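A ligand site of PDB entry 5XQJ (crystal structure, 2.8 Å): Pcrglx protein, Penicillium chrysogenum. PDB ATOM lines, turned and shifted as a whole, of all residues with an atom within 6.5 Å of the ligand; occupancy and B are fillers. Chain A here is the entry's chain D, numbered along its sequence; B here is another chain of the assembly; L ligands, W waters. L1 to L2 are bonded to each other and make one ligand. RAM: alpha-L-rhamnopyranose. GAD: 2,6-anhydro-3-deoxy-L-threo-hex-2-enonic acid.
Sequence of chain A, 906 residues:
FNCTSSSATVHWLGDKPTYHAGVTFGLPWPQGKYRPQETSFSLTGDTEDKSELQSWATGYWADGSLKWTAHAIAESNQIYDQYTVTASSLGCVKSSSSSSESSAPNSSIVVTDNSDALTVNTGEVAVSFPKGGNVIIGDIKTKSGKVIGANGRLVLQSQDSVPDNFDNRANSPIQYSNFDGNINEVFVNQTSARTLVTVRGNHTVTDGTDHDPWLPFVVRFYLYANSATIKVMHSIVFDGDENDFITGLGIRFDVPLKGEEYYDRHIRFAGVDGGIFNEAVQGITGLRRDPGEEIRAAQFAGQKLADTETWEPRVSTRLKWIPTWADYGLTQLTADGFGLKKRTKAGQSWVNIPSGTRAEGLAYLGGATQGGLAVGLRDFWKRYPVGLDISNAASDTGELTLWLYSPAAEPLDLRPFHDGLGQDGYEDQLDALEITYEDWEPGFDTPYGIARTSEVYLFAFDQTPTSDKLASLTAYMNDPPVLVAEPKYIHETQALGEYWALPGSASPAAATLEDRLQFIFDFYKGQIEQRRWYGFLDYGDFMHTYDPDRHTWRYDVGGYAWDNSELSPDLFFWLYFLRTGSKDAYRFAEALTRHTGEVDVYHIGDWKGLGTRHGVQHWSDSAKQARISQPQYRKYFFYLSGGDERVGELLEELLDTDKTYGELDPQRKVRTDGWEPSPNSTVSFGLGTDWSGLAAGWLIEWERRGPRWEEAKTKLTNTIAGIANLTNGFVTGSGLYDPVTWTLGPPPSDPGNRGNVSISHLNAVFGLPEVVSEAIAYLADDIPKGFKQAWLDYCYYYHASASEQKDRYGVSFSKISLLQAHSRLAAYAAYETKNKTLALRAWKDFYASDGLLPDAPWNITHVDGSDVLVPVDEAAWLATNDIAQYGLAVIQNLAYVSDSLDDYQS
O6B of GAD L2 is in salt-bridge range of NE of Arg 613 (2.9 Å).
The side-chain amide nitrogen (NE2) of Gln 625 is in hydrogen-bond range of an oxygen (O4) of RAM L1, 3.0 Å away.
The side-chain carboxylate (OD2) of Asp 439 lies within hydrogen-bond range of an oxygen (O1) of RAM L1, at 2.5 Å.
A ring nitrogen (NE2) of His 614 sits at hydrogen-bond distance from an oxygen (O6B) of GAD L2.
An oxygen (O6A) of GAD L2 lies within salt-bridge range of the guanidinium group of Arg 627 (3.6 Å).
The side-chain carboxylate (OE1) of Glu 566 sits close to an oxygen (O6A) of GAD L2 (2.7 Å).
Water W1 lies within hydrogen-bond range of the side-chain hydroxyl of Tyr 437 (3.0 Å), a ring nitrogen (NE2) of His 544 (3.0 Å), the side-chain carboxylate of Glu 566 (3.0 Å), the side-chain amide nitrogen of Asn 881 (3.0 Å), an oxygen (O6B) of GAD L2 (3.3 Å) and a ring nitrogen (NE2) of His 614 (3.4 Å).
The side-chain amide oxygen (OE1) of Gln 625 is in hydrogen-bond range of the guanidinium group (NH1) of Arg 627, at 3.1 Å.
The side-chain carboxylate (OD1) of Asp 621 is in hydrogen-bond range of the backbone NH (N) of Asp 439.
The side-chain carboxylate of Glu 434 lies within salt-bridge range of the guanidinium group of Arg 288 of chain B, at 3.5 Å.
OD2 of Asp 621 lies within hydrogen-bond range of N of Ala 623, 3.3 Å away.
The side-chain carboxylate (OE1) of Glu 566 is in hydrogen-bond range of a ring nitrogen (NE2) of His 614.
The side-chain carboxylate (OD1) of Asp 621 is in salt-bridge range of the guanidinium group (NH1) of Arg 613, 3.1 Å away.
O of Leu 433 sits at hydrogen-bond distance from NH1 of Arg 288 of chain B, 3.1 Å away.
The side-chain carboxylate (OE2) of Glu 566 is in salt-bridge range of the guanidinium group (NH2) of Arg 627.
CD2 of Leu 433 touches O2 of GAD L2, at 3.7 Å.
OH of Tyr 437 touches C5 of GAD L2 (3.3 Å).
Ala 623 touches the ligand.
O of Pro 666 touches C6 of RAM L1, at 3.5 Å.
OE1 of Gln 667 touches C6 of RAM L1, 3.5 Å away.
CG2 of Val 670 touches C6 of RAM L1, at 3.9 Å.
His 761 touches the ligand.
CD2 of Leu 762 touches O6A of GAD L2, 3.4 Å away.
NH2 of Arg 288 of chain B touches O2 of GAD L2, 3.9 Å away.
Hydrophobic or aromatic side chains that line the ligand: Leu 433, Tyr 437, His 614, Ala 623, Val 670, His 761 and Leu 762.
Of the 26 residues printed, 15 come within 4 Å of the ligand.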
ATOM      1  N   LEU A 430      -3.464 -10.882  18.600  1.00  0.00           N
ATOM      2  CA  LEU A 430      -4.594 -11.488  19.288  1.00  0.00           C
ATOM      3  C   LEU A 430      -4.471 -12.997  19.371  1.00  0.00           C
ATOM      4  O   LEU A 430      -5.037 -13.601  20.264  1.00  0.00           O
ATOM      5  CB  LEU A 430      -5.930 -11.101  18.620  1.00  0.00           C
ATOM      6  CG  LEU A 430      -6.349  -9.638  18.830  1.00  0.00           C
ATOM      7  CD1 LEU A 430      -7.601  -9.360  18.027  1.00  0.00           C
ATOM      8  CD2 LEU A 430      -6.597  -9.279  20.299  1.00  0.00           C
ATOM      9  N   LEU A 433      -1.969 -13.599  22.085  1.00  0.00           N
ATOM     10  CA  LEU A 433      -2.754 -13.394  23.309  1.00  0.00           C
ATOM     11  C   LEU A 433      -3.453 -14.665  23.813  1.00  0.00           C
ATOM     12  O   LEU A 433      -3.654 -14.807  24.996  1.00  0.00           O
ATOM     13  CB  LEU A 433      -3.801 -12.289  23.105  1.00  0.00           C
ATOM     14  CG  LEU A 433      -4.719 -11.929  24.299  1.00  0.00           C
ATOM     15  CD1 LEU A 433      -3.880 -11.397  25.447  1.00  0.00           C
ATOM     16  CD2 LEU A 433      -5.822 -10.946  23.893  1.00  0.00           C
ATOM     17  N   GLU A 434      -3.850 -15.549  22.900  1.00  0.00           N
ATOM     18  CA  GLU A 434      -4.549 -16.772  23.298  1.00  0.00           C
ATOM     19  C   GLU A 434      -3.614 -17.741  23.941  1.00  0.00           C
ATOM     20  O   GLU A 434      -4.122 -18.615  24.651  1.00  0.00           O
ATOM     21  CB  GLU A 434      -5.230 -17.518  22.122  1.00  0.00           C
ATOM     22  CG  GLU A 434      -6.424 -16.820  21.471  1.00  0.00           C
ATOM     23  CD  GLU A 434      -7.513 -16.402  22.443  1.00  0.00           C
ATOM     24  OE1 GLU A 434      -7.809 -17.150  23.410  1.00  0.00           O
ATOM     25  OE2 GLU A 434      -8.067 -15.307  22.242  1.00  0.00           O
ATOM     26  N   TYR A 437      -1.268 -14.944  27.156  1.00  0.00           N
ATOM     27  CA  TYR A 437      -2.104 -13.856  27.712  1.00  0.00           C
ATOM     28  C   TYR A 437      -1.482 -12.453  27.609  1.00  0.00           C
ATOM     29  O   TYR A 437      -1.924 -11.555  28.301  1.00  0.00           O
ATOM     30  CB  TYR A 437      -2.466 -14.176  29.151  1.00  0.00           C
ATOM     31  CG  TYR A 437      -3.780 -13.670  29.693  1.00  0.00           C
ATOM     32  CD1 TYR A 437      -4.944 -13.733  28.952  1.00  0.00           C
ATOM     33  CD2 TYR A 437      -3.864 -13.241  30.996  1.00  0.00           C
ATOM     34  CE1 TYR A 437      -6.158 -13.316  29.477  1.00  0.00           C
ATOM     35  CE2 TYR A 437      -5.070 -12.826  31.553  1.00  0.00           C
ATOM     36  CZ  TYR A 437      -6.229 -12.858  30.784  1.00  0.00           C
ATOM     37  OH  TYR A 437      -7.445 -12.453  31.343  1.00  0.00           O
ATOM     38  N   ASP A 439      -0.979  -9.186  25.163  1.00  0.00           N
ATOM     39  CA  ASP A 439      -1.444  -8.494  23.980  1.00  0.00           C
ATOM     40  C   ASP A 439      -0.362  -7.546  23.477  1.00  0.00           C
ATOM     41  O   ASP A 439      -0.375  -6.380  23.816  1.00  0.00           O
ATOM     42  CB  ASP A 439      -2.723  -7.719  24.318  1.00  0.00           C
ATOM     43  CG  ASP A 439      -3.301  -6.982  23.128  1.00  0.00           C
ATOM     44  OD1 ASP A 439      -2.877  -7.276  21.987  1.00  0.00           O
ATOM     45  OD2 ASP A 439      -4.190  -6.113  23.354  1.00  0.00           O
ATOM     46  N   HIS A 544       0.614 -12.519  39.072  1.00  0.00           N
ATOM     47  CA  HIS A 544      -0.773 -12.697  38.659  1.00  0.00           C
ATOM     48  C   HIS A 544      -1.217 -14.167  38.792  1.00  0.00           C
ATOM     49  O   HIS A 544      -2.023 -14.480  39.662  1.00  0.00           O
ATOM     50  CB  HIS A 544      -0.883 -12.154  37.242  1.00  0.00           C
ATOM     51  CG  HIS A 544      -2.223 -12.269  36.594  1.00  0.00           C
ATOM     52  ND1 HIS A 544      -2.653 -13.419  35.964  1.00  0.00           N
ATOM     53  CD2 HIS A 544      -3.183 -11.334  36.367  1.00  0.00           C
ATOM     54  CE1 HIS A 544      -3.842 -13.207  35.437  1.00  0.00           C
ATOM     55  NE2 HIS A 544      -4.182 -11.949  35.664  1.00  0.00           N
ATOM     56  N   GLU A 566      -4.319  -5.489  38.269  1.00  0.00           N
ATOM     57  CA  GLU A 566      -5.419  -6.251  37.641  1.00  0.00           C
ATOM     58  C   GLU A 566      -6.417  -6.816  38.661  1.00  0.00           C
ATOM     59  O   GLU A 566      -6.049  -7.554  39.602  1.00  0.00           O
ATOM     60  CB  GLU A 566      -4.852  -7.373  36.782  1.00  0.00           C
ATOM     61  CG  GLU A 566      -5.903  -8.259  36.112  1.00  0.00           C
ATOM     62  CD  GLU A 566      -6.634  -7.597  34.976  1.00  0.00           C
ATOM     63  OE1 GLU A 566      -7.279  -8.388  34.274  1.00  0.00           O
ATOM     64  OE2 GLU A 566      -6.556  -6.341  34.765  1.00  0.00           O
ATOM     65  N   LEU A 567      -7.691  -6.507  38.394  1.00  0.00           N
ATOM     66  CA  LEU A 567      -8.815  -6.701  39.315  1.00  0.00           C
ATOM     67  C   LEU A 567      -8.638  -6.109  40.716  1.00  0.00           C
ATOM     68  O   LEU A 567      -9.071  -6.668  41.684  1.00  0.00           O
ATOM     69  CB  LEU A 567      -9.282  -8.178  39.357  1.00  0.00           C
ATOM     70  CG  LEU A 567      -9.729  -8.935  38.083  1.00  0.00           C
ATOM     71  CD1 LEU A 567     -10.820  -9.962  38.385  1.00  0.00           C
ATOM     72  CD2 LEU A 567     -10.209  -8.006  36.999  1.00  0.00           C
ATOM     73  N   ARG A 613      -1.361  -2.794  31.301  1.00  0.00           N
ATOM     74  CA  ARG A 613      -1.820  -4.146  31.657  1.00  0.00           C
ATOM     75  C   ARG A 613      -0.685  -5.059  32.153  1.00  0.00           C
ATOM     76  O   ARG A 613       0.470  -5.001  31.691  1.00  0.00           O
ATOM     77  CB  ARG A 613      -2.507  -4.792  30.443  1.00  0.00           C
ATOM     78  CG  ARG A 613      -3.131  -6.138  30.692  1.00  0.00           C
ATOM     79  CD  ARG A 613      -4.095  -6.529  29.580  1.00  0.00           C
ATOM     80  NE  ARG A 613      -4.477  -7.945  29.646  1.00  0.00           N
ATOM     81  CZ  ARG A 613      -3.738  -8.949  29.183  1.00  0.00           C
ATOM     82  NH1 ARG A 613      -2.570  -8.703  28.608  1.00  0.00           N
ATOM     83  NH2 ARG A 613      -4.158 -10.221  29.292  1.00  0.00           N
ATOM     84  N   HIS A 614      -1.033  -5.881  33.145  1.00  0.00           N
ATOM     85  CA  HIS A 614      -0.160  -6.937  33.671  1.00  0.00           C
ATOM     86  C   HIS A 614       0.669  -7.668  32.631  1.00  0.00           C
ATOM     87  O   HIS A 614       0.122  -8.188  31.656  1.00  0.00           O
ATOM     88  CB  HIS A 614      -0.999  -7.949  34.433  1.00  0.00           C
ATOM     89  CG  HIS A 614      -2.212  -8.436  33.702  1.00  0.00           C
ATOM     90  ND1 HIS A 614      -2.188  -9.562  32.908  1.00  0.00           N
ATOM     91  CD2 HIS A 614      -3.488  -7.993  33.696  1.00  0.00           C
ATOM     92  CE1 HIS A 614      -3.403  -9.772  32.428  1.00  0.00           C
ATOM     93  NE2 HIS A 614      -4.215  -8.827  32.885  1.00  0.00           N
ATOM     94  N   ASP A 621       3.108  -4.694  27.846  1.00  0.00           N
ATOM     95  CA  ASP A 621       1.834  -5.030  27.177  1.00  0.00           C
ATOM     96  C   ASP A 621       1.326  -3.822  26.415  1.00  0.00           C
ATOM     97  O   ASP A 621       1.648  -2.677  26.752  1.00  0.00           O
ATOM     98  CB  ASP A 621       0.793  -5.446  28.194  1.00  0.00           C
ATOM     99  CG  ASP A 621      -0.173  -6.494  27.662  1.00  0.00           C
ATOM    100  OD1 ASP A 621       0.204  -7.700  27.787  1.00  0.00           O
ATOM    101  OD2 ASP A 621      -1.292  -6.118  27.181  1.00  0.00           O
ATOM    102  N   SER A 622       0.530  -4.063  25.366  1.00  0.00           N
ATOM    103  CA  SER A 622       0.034  -2.979  24.523  1.00  0.00           C
ATOM    104  C   SER A 622      -1.221  -2.374  25.088  1.00  0.00           C
ATOM    105  O   SER A 622      -1.578  -1.276  24.677  1.00  0.00           O
ATOM    106  CB  SER A 622      -0.215  -3.438  23.092  1.00  0.00           C
ATOM    107  OG  SER A 622      -1.484  -4.074  22.963  1.00  0.00           O
ATOM    108  N   ALA A 623      -1.888  -3.060  26.022  1.00  0.00           N
ATOM    109  CA  ALA A 623      -3.128  -2.561  26.603  1.00  0.00           C
ATOM    110  C   ALA A 623      -2.826  -1.442  27.603  1.00  0.00           C
ATOM    111  O   ALA A 623      -2.556  -1.690  28.769  1.00  0.00           O
ATOM    112  CB  ALA A 623      -3.910  -3.677  27.264  1.00  0.00           C
ATOM    113  N   GLN A 625      -4.430   1.502  29.430  1.00  0.00           N
ATOM    114  CA  GLN A 625      -5.817   1.756  29.809  1.00  0.00           C
ATOM    115  C   GLN A 625      -5.824   2.470  31.119  1.00  0.00           C
ATOM    116  O   GLN A 625      -4.909   2.306  31.905  1.00  0.00           O
ATOM    117  CB  GLN A 625      -6.609   0.471  30.006  1.00  0.00           C
ATOM    118  CG  GLN A 625      -6.762  -0.412  28.773  1.00  0.00           C
ATOM    119  CD  GLN A 625      -7.900  -1.420  28.895  1.00  0.00           C
ATOM    120  OE1 GLN A 625      -8.877  -1.221  29.660  1.00  0.00           O
ATOM    121  NE2 GLN A 625      -7.818  -2.492  28.100  1.00  0.00           N
ATOM    122  N   ARG A 627      -7.847   1.784  33.562  1.00  0.00           N
ATOM    123  CA  ARG A 627      -8.153   0.881  34.669  1.00  0.00           C
ATOM    124  C   ARG A 627      -6.905   0.538  35.534  1.00  0.00           C
ATOM    125  O   ARG A 627      -7.050   0.181  36.718  1.00  0.00           O
ATOM    126  CB  ARG A 627      -8.877  -0.354  34.169  1.00  0.00           C
ATOM    127  CG  ARG A 627      -7.993  -1.364  33.489  1.00  0.00           C
ATOM    128  CD  ARG A 627      -8.803  -2.527  32.952  1.00  0.00           C
ATOM    129  NE  ARG A 627      -7.932  -3.668  32.684  1.00  0.00           N
ATOM    130  CZ  ARG A 627      -7.917  -4.399  31.569  1.00  0.00           C
ATOM    131  NH1 ARG A 627      -8.759  -4.173  30.569  1.00  0.00           N
ATOM    132  NH2 ARG A 627      -7.066  -5.416  31.478  1.00  0.00           N
ATOM    133  N   PRO A 666      -8.358   2.123  23.295  1.00  0.00           N
ATOM    134  CA  PRO A 666      -8.083   0.866  24.047  1.00  0.00           C
ATOM    135  C   PRO A 666      -8.766  -0.380  23.462  1.00  0.00           C
ATOM    136  O   PRO A 666      -8.292  -1.503  23.666  1.00  0.00           O
ATOM    137  CB  PRO A 666      -8.674   1.151  25.426  1.00  0.00           C
ATOM    138  CG  PRO A 666      -9.783   2.109  25.155  1.00  0.00           C
ATOM    139  CD  PRO A 666      -9.204   3.016  24.100  1.00  0.00           C
ATOM    140  N   GLN A 667      -9.887  -0.154  22.767  1.00  0.00           N
ATOM    141  CA  GLN A 667     -10.674  -1.225  22.142  1.00  0.00           C
ATOM    142  C   GLN A 667     -10.319  -1.429  20.663  1.00  0.00           C
ATOM    143  O   GLN A 667     -11.069  -2.063  19.938  1.00  0.00           O
ATOM    144  CB  GLN A 667     -12.180  -0.918  22.342  1.00  0.00           C
ATOM    145  CG  GLN A 667     -12.635  -0.946  23.803  1.00  0.00           C
ATOM    146  CD  GLN A 667     -12.517  -2.344  24.398  1.00  0.00           C
ATOM    147  OE1 GLN A 667     -12.623  -3.327  23.669  1.00  0.00           O
ATOM    148  NE2 GLN A 667     -12.296  -2.436  25.698  1.00  0.00           N
ATOM    149  N   ARG A 668      -9.145  -0.946  20.237  1.00  0.00           N
ATOM    150  CA  ARG A 668      -8.808  -0.839  18.803  1.00  0.00           C
ATOM    151  C   ARG A 668      -8.721  -2.141  18.076  1.00  0.00           C
ATOM    152  O   ARG A 668      -8.911  -2.149  16.889  1.00  0.00           O
ATOM    153  CB  ARG A 668      -7.487  -0.111  18.579  1.00  0.00           C
ATOM    154  CG  ARG A 668      -6.272  -0.779  19.192  1.00  0.00           C
ATOM    155  CD  ARG A 668      -5.113   0.198  19.301  1.00  0.00           C
ATOM    156  NE  ARG A 668      -3.936  -0.390  19.952  1.00  0.00           N
ATOM    157  CZ  ARG A 668      -3.771  -0.512  21.276  1.00  0.00           C
ATOM    158  NH1 ARG A 668      -4.703  -0.098  22.141  1.00  0.00           N
ATOM    159  NH2 ARG A 668      -2.645  -1.051  21.725  1.00  0.00           N
ATOM    160  N   LYS A 669      -8.407  -3.223  18.770  1.00  0.00           N
ATOM    161  CA  LYS A 669      -8.166  -4.515  18.114  1.00  0.00           C
ATOM    162  C   LYS A 669      -9.425  -5.367  17.950  1.00  0.00           C
ATOM    163  O   LYS A 669      -9.469  -6.216  17.050  1.00  0.00           O
ATOM    164  CB  LYS A 669      -7.073  -5.301  18.882  1.00  0.00           C
ATOM    165  CG  LYS A 669      -5.886  -4.452  19.338  1.00  0.00           C
ATOM    166  CD  LYS A 669      -4.745  -5.288  19.919  1.00  0.00           C
ATOM    167  CE  LYS A 669      -3.422  -4.550  19.790  1.00  0.00           C
ATOM    168  NZ  LYS A 669      -2.218  -5.386  20.030  1.00  0.00           N
ATOM    169  N   VAL A 670     -10.433  -5.116  18.801  1.00  0.00           N
ATOM    170  CA  VAL A 670     -11.607  -6.003  18.966  1.00  0.00           C
ATOM    171  C   VAL A 670     -12.999  -5.400  18.662  1.00  0.00           C
ATOM    172  O   VAL A 670     -13.938  -6.170  18.427  1.00  0.00           O
ATOM    173  CB  VAL A 670     -11.663  -6.670  20.395  1.00  0.00           C
ATOM    174  CG1 VAL A 670     -10.428  -7.543  20.662  1.00  0.00           C
ATOM    175  CG2 VAL A 670     -11.894  -5.644  21.526  1.00  0.00           C
ATOM    176  N   THR A 689     -14.707  -0.069  32.564  1.00  0.00           N
ATOM    177  CA  THR A 689     -13.266   0.016  32.598  1.00  0.00           C
ATOM    178  C   THR A 689     -12.790   1.496  32.604  1.00  0.00           C
ATOM    179  O   THR A 689     -12.291   2.001  33.616  1.00  0.00           O
ATOM    180  CB  THR A 689     -12.631  -0.698  31.371  1.00  0.00           C
ATOM    181  OG1 THR A 689     -13.270  -0.276  30.162  1.00  0.00           O
ATOM    182  CG2 THR A 689     -12.747  -2.180  31.512  1.00  0.00           C
ATOM    183  N   HIS A 761     -17.567  -8.478  31.628  1.00  0.00           N
ATOM    184  CA  HIS A 761     -17.193  -9.012  32.936  1.00  0.00           C
ATOM    185  C   HIS A 761     -16.113  -8.141  33.631  1.00  0.00           C
ATOM    186  O   HIS A 761     -15.992  -8.176  34.857  1.00  0.00           O
ATOM    187  CB  HIS A 761     -16.812 -10.509  32.813  1.00  0.00           C
ATOM    188  CG  HIS A 761     -15.440 -10.786  32.264  1.00  0.00           C
ATOM    189  ND1 HIS A 761     -15.163 -10.773  30.915  1.00  0.00           N
ATOM    190  CD2 HIS A 761     -14.285 -11.139  32.875  1.00  0.00           C
ATOM    191  CE1 HIS A 761     -13.891 -11.070  30.722  1.00  0.00           C
ATOM    192  NE2 HIS A 761     -13.330 -11.302  31.895  1.00  0.00           N
ATOM    193  N   LEU A 762     -15.389  -7.335  32.846  1.00  0.00           N
ATOM    194  CA  LEU A 762     -14.414  -6.385  33.404  1.00  0.00           C
ATOM    195  C   LEU A 762     -14.999  -5.067  33.901  1.00  0.00           C
ATOM    196  O   LEU A 762     -14.386  -4.394  34.711  1.00  0.00           O
ATOM    197  CB  LEU A 762     -13.343  -6.071  32.355  1.00  0.00           C
ATOM    198  CG  LEU A 762     -12.595  -7.289  31.821  1.00  0.00           C
ATOM    199  CD1 LEU A 762     -11.688  -6.876  30.672  1.00  0.00           C
ATOM    200  CD2 LEU A 762     -11.831  -8.007  32.948  1.00  0.00           C
ATOM    201  N   PHE A 766     -12.968  -2.749  38.525  1.00  0.00           N
ATOM    202  CA  PHE A 766     -11.816  -1.861  38.583  1.00  0.00           C
ATOM    203  C   PHE A 766     -12.116  -0.549  39.276  1.00  0.00           C
ATOM    204  O   PHE A 766     -11.515   0.480  38.993  1.00  0.00           O
ATOM    205  CB  PHE A 766     -11.310  -1.607  37.159  1.00  0.00           C
ATOM    206  CG  PHE A 766     -10.701  -2.809  36.505  1.00  0.00           C
ATOM    207  CD1 PHE A 766     -11.491  -3.676  35.760  1.00  0.00           C
ATOM    208  CD2 PHE A 766      -9.342  -3.072  36.594  1.00  0.00           C
ATOM    209  CE1 PHE A 766     -10.935  -4.788  35.122  1.00  0.00           C
ATOM    210  CE2 PHE A 766      -8.779  -4.178  35.967  1.00  0.00           C
ATOM    211  CZ  PHE A 766      -9.577  -5.045  35.227  1.00  0.00           C
ATOM    212  N   ASN A 881      -6.242 -12.606  40.612  1.00  0.00           N
ATOM    213  CA  ASN A 881      -7.625 -12.199  40.219  1.00  0.00           C
ATOM    214  C   ASN A 881      -8.656 -12.684  41.211  1.00  0.00           C
ATOM    215  O   ASN A 881      -9.525 -11.895  41.591  1.00  0.00           O
ATOM    216  CB  ASN A 881      -7.996 -12.663  38.804  1.00  0.00           C
ATOM    217  CG  ASN A 881      -7.314 -11.843  37.755  1.00  0.00           C
ATOM    218  OD1 ASN A 881      -6.576 -10.920  38.095  1.00  0.00           O
ATOM    219  ND2 ASN A 881      -7.520 -12.160  36.507  1.00  0.00           N
ATOM    220  N   ARG B 288      -1.714 -19.981  28.967  1.00  0.00           N
ATOM    221  CA  ARG B 288      -3.177 -19.792  29.081  1.00  0.00           C
ATOM    222  C   ARG B 288      -3.958 -21.066  28.783  1.00  0.00           C
ATOM    223  O   ARG B 288      -5.051 -21.263  29.331  1.00  0.00           O
ATOM    224  CB  ARG B 288      -3.642 -18.662  28.123  1.00  0.00           C
ATOM    225  CG  ARG B 288      -5.142 -18.313  28.170  1.00  0.00           C
ATOM    226  CD  ARG B 288      -5.450 -17.094  27.330  1.00  0.00           C
ATOM    227  NE  ARG B 288      -6.814 -16.589  27.504  1.00  0.00           N
ATOM    228  CZ  ARG B 288      -7.343 -15.572  26.807  1.00  0.00           C
ATOM    229  NH1 ARG B 288      -6.626 -14.918  25.875  1.00  0.00           N
ATOM    230  NH2 ARG B 288      -8.590 -15.176  27.044  1.00  0.00           N
HETATM  231  C1  RAM L   1      -6.799  -6.926  25.532  1.00  0.00           C
HETATM  232  C2  RAM L   1      -7.138  -7.188  27.010  1.00  0.00           C
HETATM  233  C3  RAM L   1      -7.939  -6.060  27.677  1.00  0.00           C
HETATM  234  C4  RAM L   1      -9.092  -5.564  26.783  1.00  0.00           C
HETATM  235  C5  RAM L   1      -8.482  -5.128  25.455  1.00  0.00           C
HETATM  236  C6  RAM L   1      -9.532  -4.670  24.461  1.00  0.00           C
HETATM  237  O1  RAM L   1      -5.536  -6.253  25.437  1.00  0.00           O
HETATM  238  O2  RAM L   1      -7.836  -8.462  27.187  1.00  0.00           O
HETATM  239  O3  RAM L   1      -8.400  -6.581  28.916  1.00  0.00           O
HETATM  240  O4  RAM L   1      -9.890  -4.511  27.414  1.00  0.00           O
HETATM  241  O5  RAM L   1      -7.831  -6.214  24.817  1.00  0.00           O
HETATM  242  C1  GAD L   2      -7.598  -9.798  27.420  1.00  0.00           C
HETATM  243  C2  GAD L   2      -8.545 -11.008  27.458  1.00  0.00           C
HETATM  244  O2  GAD L   2      -8.766 -11.431  26.091  1.00  0.00           O
HETATM  245  C3  GAD L   2      -9.788 -10.661  28.318  1.00  0.00           C
HETATM  246  O3  GAD L   2     -10.756 -11.693  28.444  1.00  0.00           O
HETATM  247  C4  GAD L   2      -9.355 -10.257  29.716  1.00  0.00           C
HETATM  248  C5  GAD L   2      -8.160  -9.616  29.898  1.00  0.00           C
HETATM  249  C6  GAD L   2      -7.760  -9.036  31.181  1.00  0.00           C
HETATM  250  O6A GAD L   2      -8.624  -8.590  31.951  1.00  0.00           O
HETATM  251  O6B GAD L   2      -6.533  -8.954  31.435  1.00  0.00           O
HETATM  252  O5  GAD L   2      -7.239  -9.420  28.776  1.00  0.00           O
HETATM  253  O   HOH W   1      -6.441 -11.219  33.861  1.00  0.00           O
